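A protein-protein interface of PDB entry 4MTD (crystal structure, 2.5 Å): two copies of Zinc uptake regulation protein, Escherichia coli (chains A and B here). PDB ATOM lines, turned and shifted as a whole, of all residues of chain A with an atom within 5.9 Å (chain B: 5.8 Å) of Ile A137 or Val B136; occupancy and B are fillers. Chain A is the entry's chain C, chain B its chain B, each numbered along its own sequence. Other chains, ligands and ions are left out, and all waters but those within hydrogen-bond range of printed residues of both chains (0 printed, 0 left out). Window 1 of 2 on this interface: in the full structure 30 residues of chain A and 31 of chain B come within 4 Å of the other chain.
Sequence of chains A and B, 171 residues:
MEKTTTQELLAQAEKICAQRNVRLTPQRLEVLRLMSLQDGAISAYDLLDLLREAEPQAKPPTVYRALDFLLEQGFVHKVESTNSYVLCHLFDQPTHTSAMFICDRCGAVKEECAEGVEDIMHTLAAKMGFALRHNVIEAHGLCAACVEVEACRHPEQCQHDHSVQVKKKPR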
ATOM      1  N   SER A  81     -10.911   6.308  -2.614  1.00  0.00           N
ATOM      2  CA  SER A  81     -10.192   6.300  -1.345  1.00  0.00           C
ATOM      3  C   SER A  81      -8.961   7.219  -1.273  1.00  0.00           C
ATOM      4  O   SER A  81      -8.296   7.271  -0.239  1.00  0.00           O
ATOM      5  CB  SER A  81      -9.785   4.863  -0.990  1.00  0.00           C
ATOM      6  OG  SER A  81      -8.764   4.370  -1.848  1.00  0.00           O
ATOM      7  N   THR A  97     -16.086  -2.677 -14.450  1.00  0.00           N
ATOM      8  CA  THR A  97     -15.781  -2.262 -13.092  1.00  0.00           C
ATOM      9  C   THR A  97     -14.317  -2.556 -12.808  1.00  0.00           C
ATOM     10  O   THR A  97     -13.910  -3.711 -12.717  1.00  0.00           O
ATOM     11  CB  THR A  97     -16.656  -2.981 -12.058  1.00  0.00           C
ATOM     12  OG1 THR A  97     -18.002  -3.059 -12.542  1.00  0.00           O
ATOM     13  CG2 THR A  97     -16.633  -2.236 -10.727  1.00  0.00           C
ATOM     14  N   SER A  98     -13.539  -1.488 -12.675  1.00  0.00           N
ATOM     15  CA  SER A  98     -12.135  -1.581 -12.311  1.00  0.00           C
ATOM     16  C   SER A  98     -11.980  -1.987 -10.855  1.00  0.00           C
ATOM     17  O   SER A  98     -12.826  -1.677 -10.029  1.00  0.00           O
ATOM     18  CB  SER A  98     -11.484  -0.221 -12.505  1.00  0.00           C
ATOM     19  OG  SER A  98     -12.192   0.769 -11.770  1.00  0.00           O
ATOM     20  N   ALA A  99     -10.898  -2.692 -10.553  1.00  0.00           N
ATOM     21  CA  ALA A  99     -10.473  -2.910  -9.185  1.00  0.00           C
ATOM     22  C   ALA A  99      -9.074  -2.303  -9.052  1.00  0.00           C
ATOM     23  O   ALA A  99      -8.118  -2.825  -9.629  1.00  0.00           O
ATOM     24  CB  ALA A  99     -10.453  -4.394  -8.872  1.00  0.00           C
ATOM     25  N   MET A 100      -8.960  -1.202  -8.309  1.00  0.00           N
ATOM     26  CA  MET A 100      -7.725  -0.402  -8.283  1.00  0.00           C
ATOM     27  C   MET A 100      -6.814  -0.801  -7.129  1.00  0.00           C
ATOM     28  O   MET A 100      -7.185  -0.675  -5.963  1.00  0.00           O
ATOM     29  CB  MET A 100      -8.044   1.095  -8.166  1.00  0.00           C
ATOM     30  CG  MET A 100      -8.825   1.687  -9.333  1.00  0.00           C
ATOM     31  SD  MET A 100      -7.867   1.708 -10.860  1.00  0.00           S
ATOM     32  CE  MET A 100      -8.972   2.538 -11.993  1.00  0.00           C
ATOM     33  N   PHE A 101      -5.622  -1.277  -7.461  1.00  0.00           N
ATOM     34  CA  PHE A 101      -4.608  -1.569  -6.465  1.00  0.00           C
ATOM     35  C   PHE A 101      -3.717  -0.359  -6.309  1.00  0.00           C
ATOM     36  O   PHE A 101      -3.161   0.136  -7.286  1.00  0.00           O
ATOM     37  CB  PHE A 101      -3.815  -2.804  -6.869  1.00  0.00           C
ATOM     38  CG  PHE A 101      -4.605  -4.056  -6.728  1.00  0.00           C
ATOM     39  CD1 PHE A 101      -4.444  -4.866  -5.624  1.00  0.00           C
ATOM     40  CD2 PHE A 101      -5.569  -4.376  -7.661  1.00  0.00           C
ATOM     41  CE1 PHE A 101      -5.196  -6.006  -5.473  1.00  0.00           C
ATOM     42  CE2 PHE A 101      -6.334  -5.506  -7.518  1.00  0.00           C
ATOM     43  CZ  PHE A 101      -6.149  -6.322  -6.421  1.00  0.00           C
ATOM     44  N   ALA A 114     -11.800  -7.821 -11.665  1.00  0.00           N
ATOM     45  CA  ALA A 114     -12.163  -8.708 -10.566  1.00  0.00           C
ATOM     46  C   ALA A 114     -13.644  -9.090 -10.625  1.00  0.00           C
ATOM     47  O   ALA A 114     -14.434  -8.723  -9.753  1.00  0.00           O
ATOM     48  CB  ALA A 114     -11.823  -8.053  -9.238  1.00  0.00           C
ATOM     49  N   VAL A 117     -15.335 -10.665  -7.615  1.00  0.00           N
ATOM     50  CA  VAL A 117     -15.803  -9.785  -6.552  1.00  0.00           C
ATOM     51  C   VAL A 117     -17.151  -9.183  -6.932  1.00  0.00           C
ATOM     52  O   VAL A 117     -18.065  -9.159  -6.123  1.00  0.00           O
ATOM     53  CB  VAL A 117     -14.774  -8.672  -6.236  1.00  0.00           C
ATOM     54  CG1 VAL A 117     -15.321  -7.705  -5.197  1.00  0.00           C
ATOM     55  CG2 VAL A 117     -13.469  -9.279  -5.736  1.00  0.00           C
ATOM     56  N   GLU A 118     -17.273  -8.725  -8.171  1.00  0.00           N
ATOM     57  CA  GLU A 118     -18.537  -8.186  -8.668  1.00  0.00           C
ATOM     58  C   GLU A 118     -19.655  -9.238  -8.615  1.00  0.00           C
ATOM     59  O   GLU A 118     -20.761  -8.945  -8.150  1.00  0.00           O
ATOM     60  CB  GLU A 118     -18.380  -7.680 -10.100  1.00  0.00           C
ATOM     61  CG  GLU A 118     -17.329  -6.596 -10.276  1.00  0.00           C
ATOM     62  CD  GLU A 118     -17.042  -6.319 -11.733  1.00  0.00           C
ATOM     63  OE1 GLU A 118     -18.003  -6.017 -12.466  1.00  0.00           O
ATOM     64  OE2 GLU A 118     -15.863  -6.393 -12.149  1.00  0.00           O
ATOM     65  N   MET A 121     -20.790  -9.600  -5.137  1.00  0.00           N
ATOM     66  CA  MET A 121     -21.498  -8.397  -4.710  1.00  0.00           C
ATOM     67  C   MET A 121     -22.935  -8.437  -5.208  1.00  0.00           C
ATOM     68  O   MET A 121     -23.866  -8.195  -4.442  1.00  0.00           O
ATOM     69  CB  MET A 121     -20.793  -7.137  -5.239  1.00  0.00           C
ATOM     70  CG  MET A 121     -20.593  -6.028  -4.213  1.00  0.00           C
ATOM     71  SD  MET A 121     -19.636  -6.478  -2.750  1.00  0.00           S
ATOM     72  CE  MET A 121     -18.236  -7.260  -3.532  1.00  0.00           C
ATOM     73  N   ASN A 135     -20.217  -0.700  -8.375  1.00  0.00           N
ATOM     74  CA  ASN A 135     -19.316  -1.180  -7.352  1.00  0.00           C
ATOM     75  C   ASN A 135     -18.012  -0.390  -7.333  1.00  0.00           C
ATOM     76  O   ASN A 135     -17.455  -0.070  -8.377  1.00  0.00           O
ATOM     77  CB  ASN A 135     -18.990  -2.642  -7.609  1.00  0.00           C
ATOM     78  CG  ASN A 135     -20.104  -3.565  -7.190  1.00  0.00           C
ATOM     79  OD1 ASN A 135     -20.629  -3.458  -6.081  1.00  0.00           O
ATOM     80  ND2 ASN A 135     -20.460  -4.486  -8.065  1.00  0.00           N
ATOM     81  N   VAL A 136     -17.544  -0.085  -6.128  1.00  0.00           N
ATOM     82  CA  VAL A 136     -16.245   0.513  -5.909  1.00  0.00           C
ATOM     83  C   VAL A 136     -15.411  -0.572  -5.256  1.00  0.00           C
ATOM     84  O   VAL A 136     -15.823  -1.123  -4.234  1.00  0.00           O
ATOM     85  CB  VAL A 136     -16.348   1.739  -4.981  1.00  0.00           C
ATOM     86  CG1 VAL A 136     -14.962   2.301  -4.656  1.00  0.00           C
ATOM     87  CG2 VAL A 136     -17.241   2.805  -5.616  1.00  0.00           C
ATOM     88  N   ILE A 137     -14.271  -0.897  -5.880  1.00  0.00           N
ATOM     89  CA  ILE A 137     -13.350  -1.940  -5.405  1.00  0.00           C
ATOM     90  C   ILE A 137     -11.923  -1.401  -5.478  1.00  0.00           C
ATOM     91  O   ILE A 137     -11.424  -1.095  -6.558  1.00  0.00           O
ATOM     92  CB  ILE A 137     -13.450  -3.225  -6.259  1.00  0.00           C
ATOM     93  CG1 ILE A 137     -14.889  -3.768  -6.262  1.00  0.00           C
ATOM     94  CG2 ILE A 137     -12.503  -4.304  -5.732  1.00  0.00           C
ATOM     95  CD1 ILE A 137     -15.175  -4.772  -7.360  1.00  0.00           C
ATOM     96  N   GLU A 138     -11.282  -1.269  -4.320  1.00  0.00           N
ATOM     97  CA  GLU A 138      -9.983  -0.617  -4.197  1.00  0.00           C
ATOM     98  C   GLU A 138      -9.163  -1.333  -3.135  1.00  0.00           C
ATOM     99  O   GLU A 138      -9.672  -1.682  -2.077  1.00  0.00           O
ATOM    100  CB  GLU A 138     -10.150   0.869  -3.841  1.00  0.00           C
ATOM    101  CG  GLU A 138     -10.832   1.687  -4.936  1.00  0.00           C
ATOM    102  CD  GLU A 138     -11.041   3.164  -4.595  1.00  0.00           C
ATOM    103  OE1 GLU A 138     -10.568   3.627  -3.546  1.00  0.00           O
ATOM    104  OE2 GLU A 138     -11.688   3.884  -5.389  1.00  0.00           O
ATOM    105  N   ALA A 139      -7.893  -1.576  -3.428  1.00  0.00           N
ATOM    106  CA  ALA A 139      -6.989  -2.169  -2.449  1.00  0.00           C
ATOM    107  C   ALA A 139      -5.847  -1.206  -2.169  1.00  0.00           C
ATOM    108  O   ALA A 139      -5.351  -0.553  -3.075  1.00  0.00           O
ATOM    109  CB  ALA A 139      -6.449  -3.498  -2.960  1.00  0.00           C
ATOM    110  N   HIS A 140      -5.453  -1.135  -0.904  1.00  0.00           N
ATOM    111  CA  HIS A 140      -4.304  -0.364  -0.456  1.00  0.00           C
ATOM    112  C   HIS A 140      -3.231  -1.316   0.035  1.00  0.00           C
ATOM    113  O   HIS A 140      -3.529  -2.325   0.702  1.00  0.00           O
ATOM    114  CB  HIS A 140      -4.683   0.583   0.686  1.00  0.00           C
ATOM    115  CG  HIS A 140      -5.427   1.793   0.230  1.00  0.00           C
ATOM    116  ND1 HIS A 140      -4.798   2.979  -0.075  1.00  0.00           N
ATOM    117  CD2 HIS A 140      -6.746   1.993  -0.004  1.00  0.00           C
ATOM    118  CE1 HIS A 140      -5.696   3.861  -0.471  1.00  0.00           C
ATOM    119  NE2 HIS A 140      -6.886   3.287  -0.441  1.00  0.00           N
ATOM    120  N   GLU B  80     -15.530   5.415   2.107  1.00  0.00           N
ATOM    121  CA  GLU B  80     -14.637   6.256   1.306  1.00  0.00           C
ATOM    122  C   GLU B  80     -15.349   6.977   0.180  1.00  0.00           C
ATOM    123  O   GLU B  80     -15.010   8.108  -0.142  1.00  0.00           O
ATOM    124  CB  GLU B  80     -13.512   5.410   0.713  1.00  0.00           C
ATOM    125  CG  GLU B  80     -12.618   4.738   1.747  1.00  0.00           C
ATOM    126  CD  GLU B  80     -11.679   5.710   2.437  1.00  0.00           C
ATOM    127  OE1 GLU B  80     -11.590   6.876   2.004  1.00  0.00           O
ATOM    128  OE2 GLU B  80     -11.021   5.298   3.409  1.00  0.00           O
ATOM    129  N   MET B 121      -9.237 -11.014  -3.724  1.00  0.00           N
ATOM    130  CA  MET B 121      -8.320  -9.879  -3.744  1.00  0.00           C
ATOM    131  C   MET B 121      -6.897 -10.286  -3.344  1.00  0.00           C
ATOM    132  O   MET B 121      -5.922  -9.764  -3.884  1.00  0.00           O
ATOM    133  CB  MET B 121      -8.814  -8.774  -2.806  1.00  0.00           C
ATOM    134  CG  MET B 121     -10.137  -8.139  -3.204  1.00  0.00           C
ATOM    135  SD  MET B 121     -10.095  -7.291  -4.791  1.00  0.00           S
ATOM    136  CE  MET B 121      -9.165  -5.817  -4.360  1.00  0.00           C
ATOM    137  N   HIS B 134      -5.431  -3.314   3.153  1.00  0.00           N
ATOM    138  CA  HIS B 134      -6.861  -3.076   3.336  1.00  0.00           C
ATOM    139  C   HIS B 134      -7.581  -3.137   2.006  1.00  0.00           C
ATOM    140  O   HIS B 134      -7.019  -2.794   0.968  1.00  0.00           O
ATOM    141  CB  HIS B 134      -7.134  -1.693   3.949  1.00  0.00           C
ATOM    142  CG  HIS B 134      -6.333  -1.392   5.177  1.00  0.00           C
ATOM    143  ND1 HIS B 134      -5.160  -0.666   5.141  1.00  0.00           N
ATOM    144  CD2 HIS B 134      -6.545  -1.698   6.480  1.00  0.00           C
ATOM    145  CE1 HIS B 134      -4.679  -0.549   6.366  1.00  0.00           C
ATOM    146  NE2 HIS B 134      -5.500  -1.165   7.197  1.00  0.00           N
ATOM    147  N   ASN B 135      -8.842  -3.554   2.060  1.00  0.00           N
ATOM    148  CA  ASN B 135      -9.725  -3.520   0.912  1.00  0.00           C
ATOM    149  C   ASN B 135     -10.828  -2.494   1.141  1.00  0.00           C
ATOM    150  O   ASN B 135     -11.321  -2.335   2.250  1.00  0.00           O
ATOM    151  CB  ASN B 135     -10.328  -4.911   0.656  1.00  0.00           C
ATOM    152  CG  ASN B 135      -9.287  -5.927   0.212  1.00  0.00           C
ATOM    153  OD1 ASN B 135      -9.001  -6.894   0.917  1.00  0.00           O
ATOM    154  ND2 ASN B 135      -8.709  -5.706  -0.957  1.00  0.00           N
ATOM    155  N   VAL B 136     -11.185  -1.786   0.080  1.00  0.00           N
ATOM    156  CA  VAL B 136     -12.283  -0.844   0.090  1.00  0.00           C
ATOM    157  C   VAL B 136     -13.281  -1.388  -0.916  1.00  0.00           C
ATOM    158  O   VAL B 136     -12.983  -1.484  -2.108  1.00  0.00           O
ATOM    159  CB  VAL B 136     -11.812   0.564  -0.318  1.00  0.00           C
ATOM    160  CG1 VAL B 136     -12.988   1.525  -0.427  1.00  0.00           C
ATOM    161  CG2 VAL B 136     -10.787   1.086   0.680  1.00  0.00           C
ATOM    162  N   ILE B 137     -14.453  -1.771  -0.424  1.00  0.00           N
ATOM    163  CA  ILE B 137     -15.447  -2.479  -1.217  1.00  0.00           C
ATOM    164  C   ILE B 137     -16.805  -1.898  -0.901  1.00  0.00           C
ATOM    165  O   ILE B 137     -17.351  -2.119   0.180  1.00  0.00           O
ATOM    166  CB  ILE B 137     -15.432  -3.979  -0.881  1.00  0.00           C
ATOM    167  CG1 ILE B 137     -14.153  -4.616  -1.418  1.00  0.00           C
ATOM    168  CG2 ILE B 137     -16.639  -4.695  -1.469  1.00  0.00           C
ATOM    169  CD1 ILE B 137     -13.700  -5.747  -0.541  1.00  0.00           C
ATOM    170  N   GLU B 138     -17.345  -1.141  -1.843  1.00  0.00           N
ATOM    171  CA  GLU B 138     -18.543  -0.370  -1.581  1.00  0.00           C
ATOM    172  C   GLU B 138     -19.463  -0.483  -2.784  1.00  0.00           C
ATOM    173  O   GLU B 138     -19.023  -0.364  -3.916  1.00  0.00           O
ATOM    174  CB  GLU B 138     -18.163   1.085  -1.250  1.00  0.00           C
ATOM    175  CG  GLU B 138     -17.116   1.164  -0.130  1.00  0.00           C
ATOM    176  CD  GLU B 138     -16.691   2.569   0.280  1.00  0.00           C
ATOM    177  OE1 GLU B 138     -16.948   3.547  -0.467  1.00  0.00           O
ATOM    178  OE2 GLU B 138     -16.071   2.677   1.366  1.00  0.00           O
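Met A121 touches Ile B137, and with the chains exchanged Ile A137 touches Met B121. Asn A135 touches Glu B138, and with the chains exchanged Glu A138 touches Asn B135. Val A136 touches Ile B137, and with the chains exchanged Ile A137 touches Val B136. Val A136 touches Glu B138, and with the chains exchanged Glu A138 touches Val B136. Positions printed for both chains: 121, 135, 136, 137 and 138.
The side-chain carboxylate (OE2) of Glu B138 lies within hydrogen-bond range of the backbone NH (N) of Glu B80, 2.9 Å away. The side-chain hydroxyl (OG) of Ser A81 sits at hydrogen-bond distance from a ring nitrogen (NE2) of His A140 (2.6 Å). O of Met A100 sits at hydrogen-bond distance from N of Ala A139 (2.8 Å). N of Met A100 is in hydrogen-bond range of O of Ile A137, 3.0 Å away. The side-chain hydroxyl (OG) of Ser A81 is in hydrogen-bond range of the side-chain carboxylate (OE1) of Glu A138, at 2.6 Å.
The backbone NH of Val B136 is in hydrogen-bond range of the backbone carbonyl oxygen of Glu A138 (2.6 Å). O of Glu B138 lies within hydrogen-bond range of N of Val A136, at 2.7 Å. The backbone carbonyl oxygen of His B134 lies within hydrogen-bond range of the backbone NH of His A140 (3.0 Å).
Printed residues of chain B within 4 Å of Asn A135: Glu B138 (3.5 Å). Printed residues of chain B within 4 Å of Ile A137: Met B121 and Val B136. Of the printed residues of chain B, Ala A139 touches Met B121 (3.8 Å), His B134 (3.5 Å) and Asn B135 (3.7 Å). Of the printed residues of chain A, Met B121 touches Phe A101, Ile A137 and Ala A139. Of the printed residues of chain A, His B134 touches Ala A139 and His A140. Val B136 touches just these residues of chain A: Val A136 (3.6 Å), Ile A137 (3.3 Å) and Glu A138 (2.6 Å). Of the printed residues of chain A, Glu B138 touches Asn A135 (3.5 Å) and Val A136 (2.7 Å). The nearest residue of chain B that does not touch Ile A137 is Ile B137 (4.6 Å). The nearest printed residue of chain B that does not touch His A140 is Val B136 (4.2 Å).
Met B121 touches Phe A101 (CE to CZ, 3.7 Å). Met A121 touches Ile B137. Asn A135 touches Glu B138. Val A136 touches Val B136 (O to O, 3.6 Å). Val A136 touches Ile B137 (O to CA, 3.3 Å). Met B121 touches Ile A137 (CE to CG2, 3.9 Å). O of Val B136 touches CA of Ile A137, at 3.3 Å. O of Glu A138 touches CA of Asn B135 (3.5 Å). Ala A139 touches Met B121 (CB to CE, 3.8 Å). Ala A139 touches Asn B135 (CB to ND2, 3.7 Å).
Hydrophobic or aromatic side chains of chain A within 4 Å of the printed part of chain B: Phe A101, Met A121, Val A136, Ile A137 and Ala A139. Of the 7 printed residues of chain B, 7 touch a printed residue of chain A.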
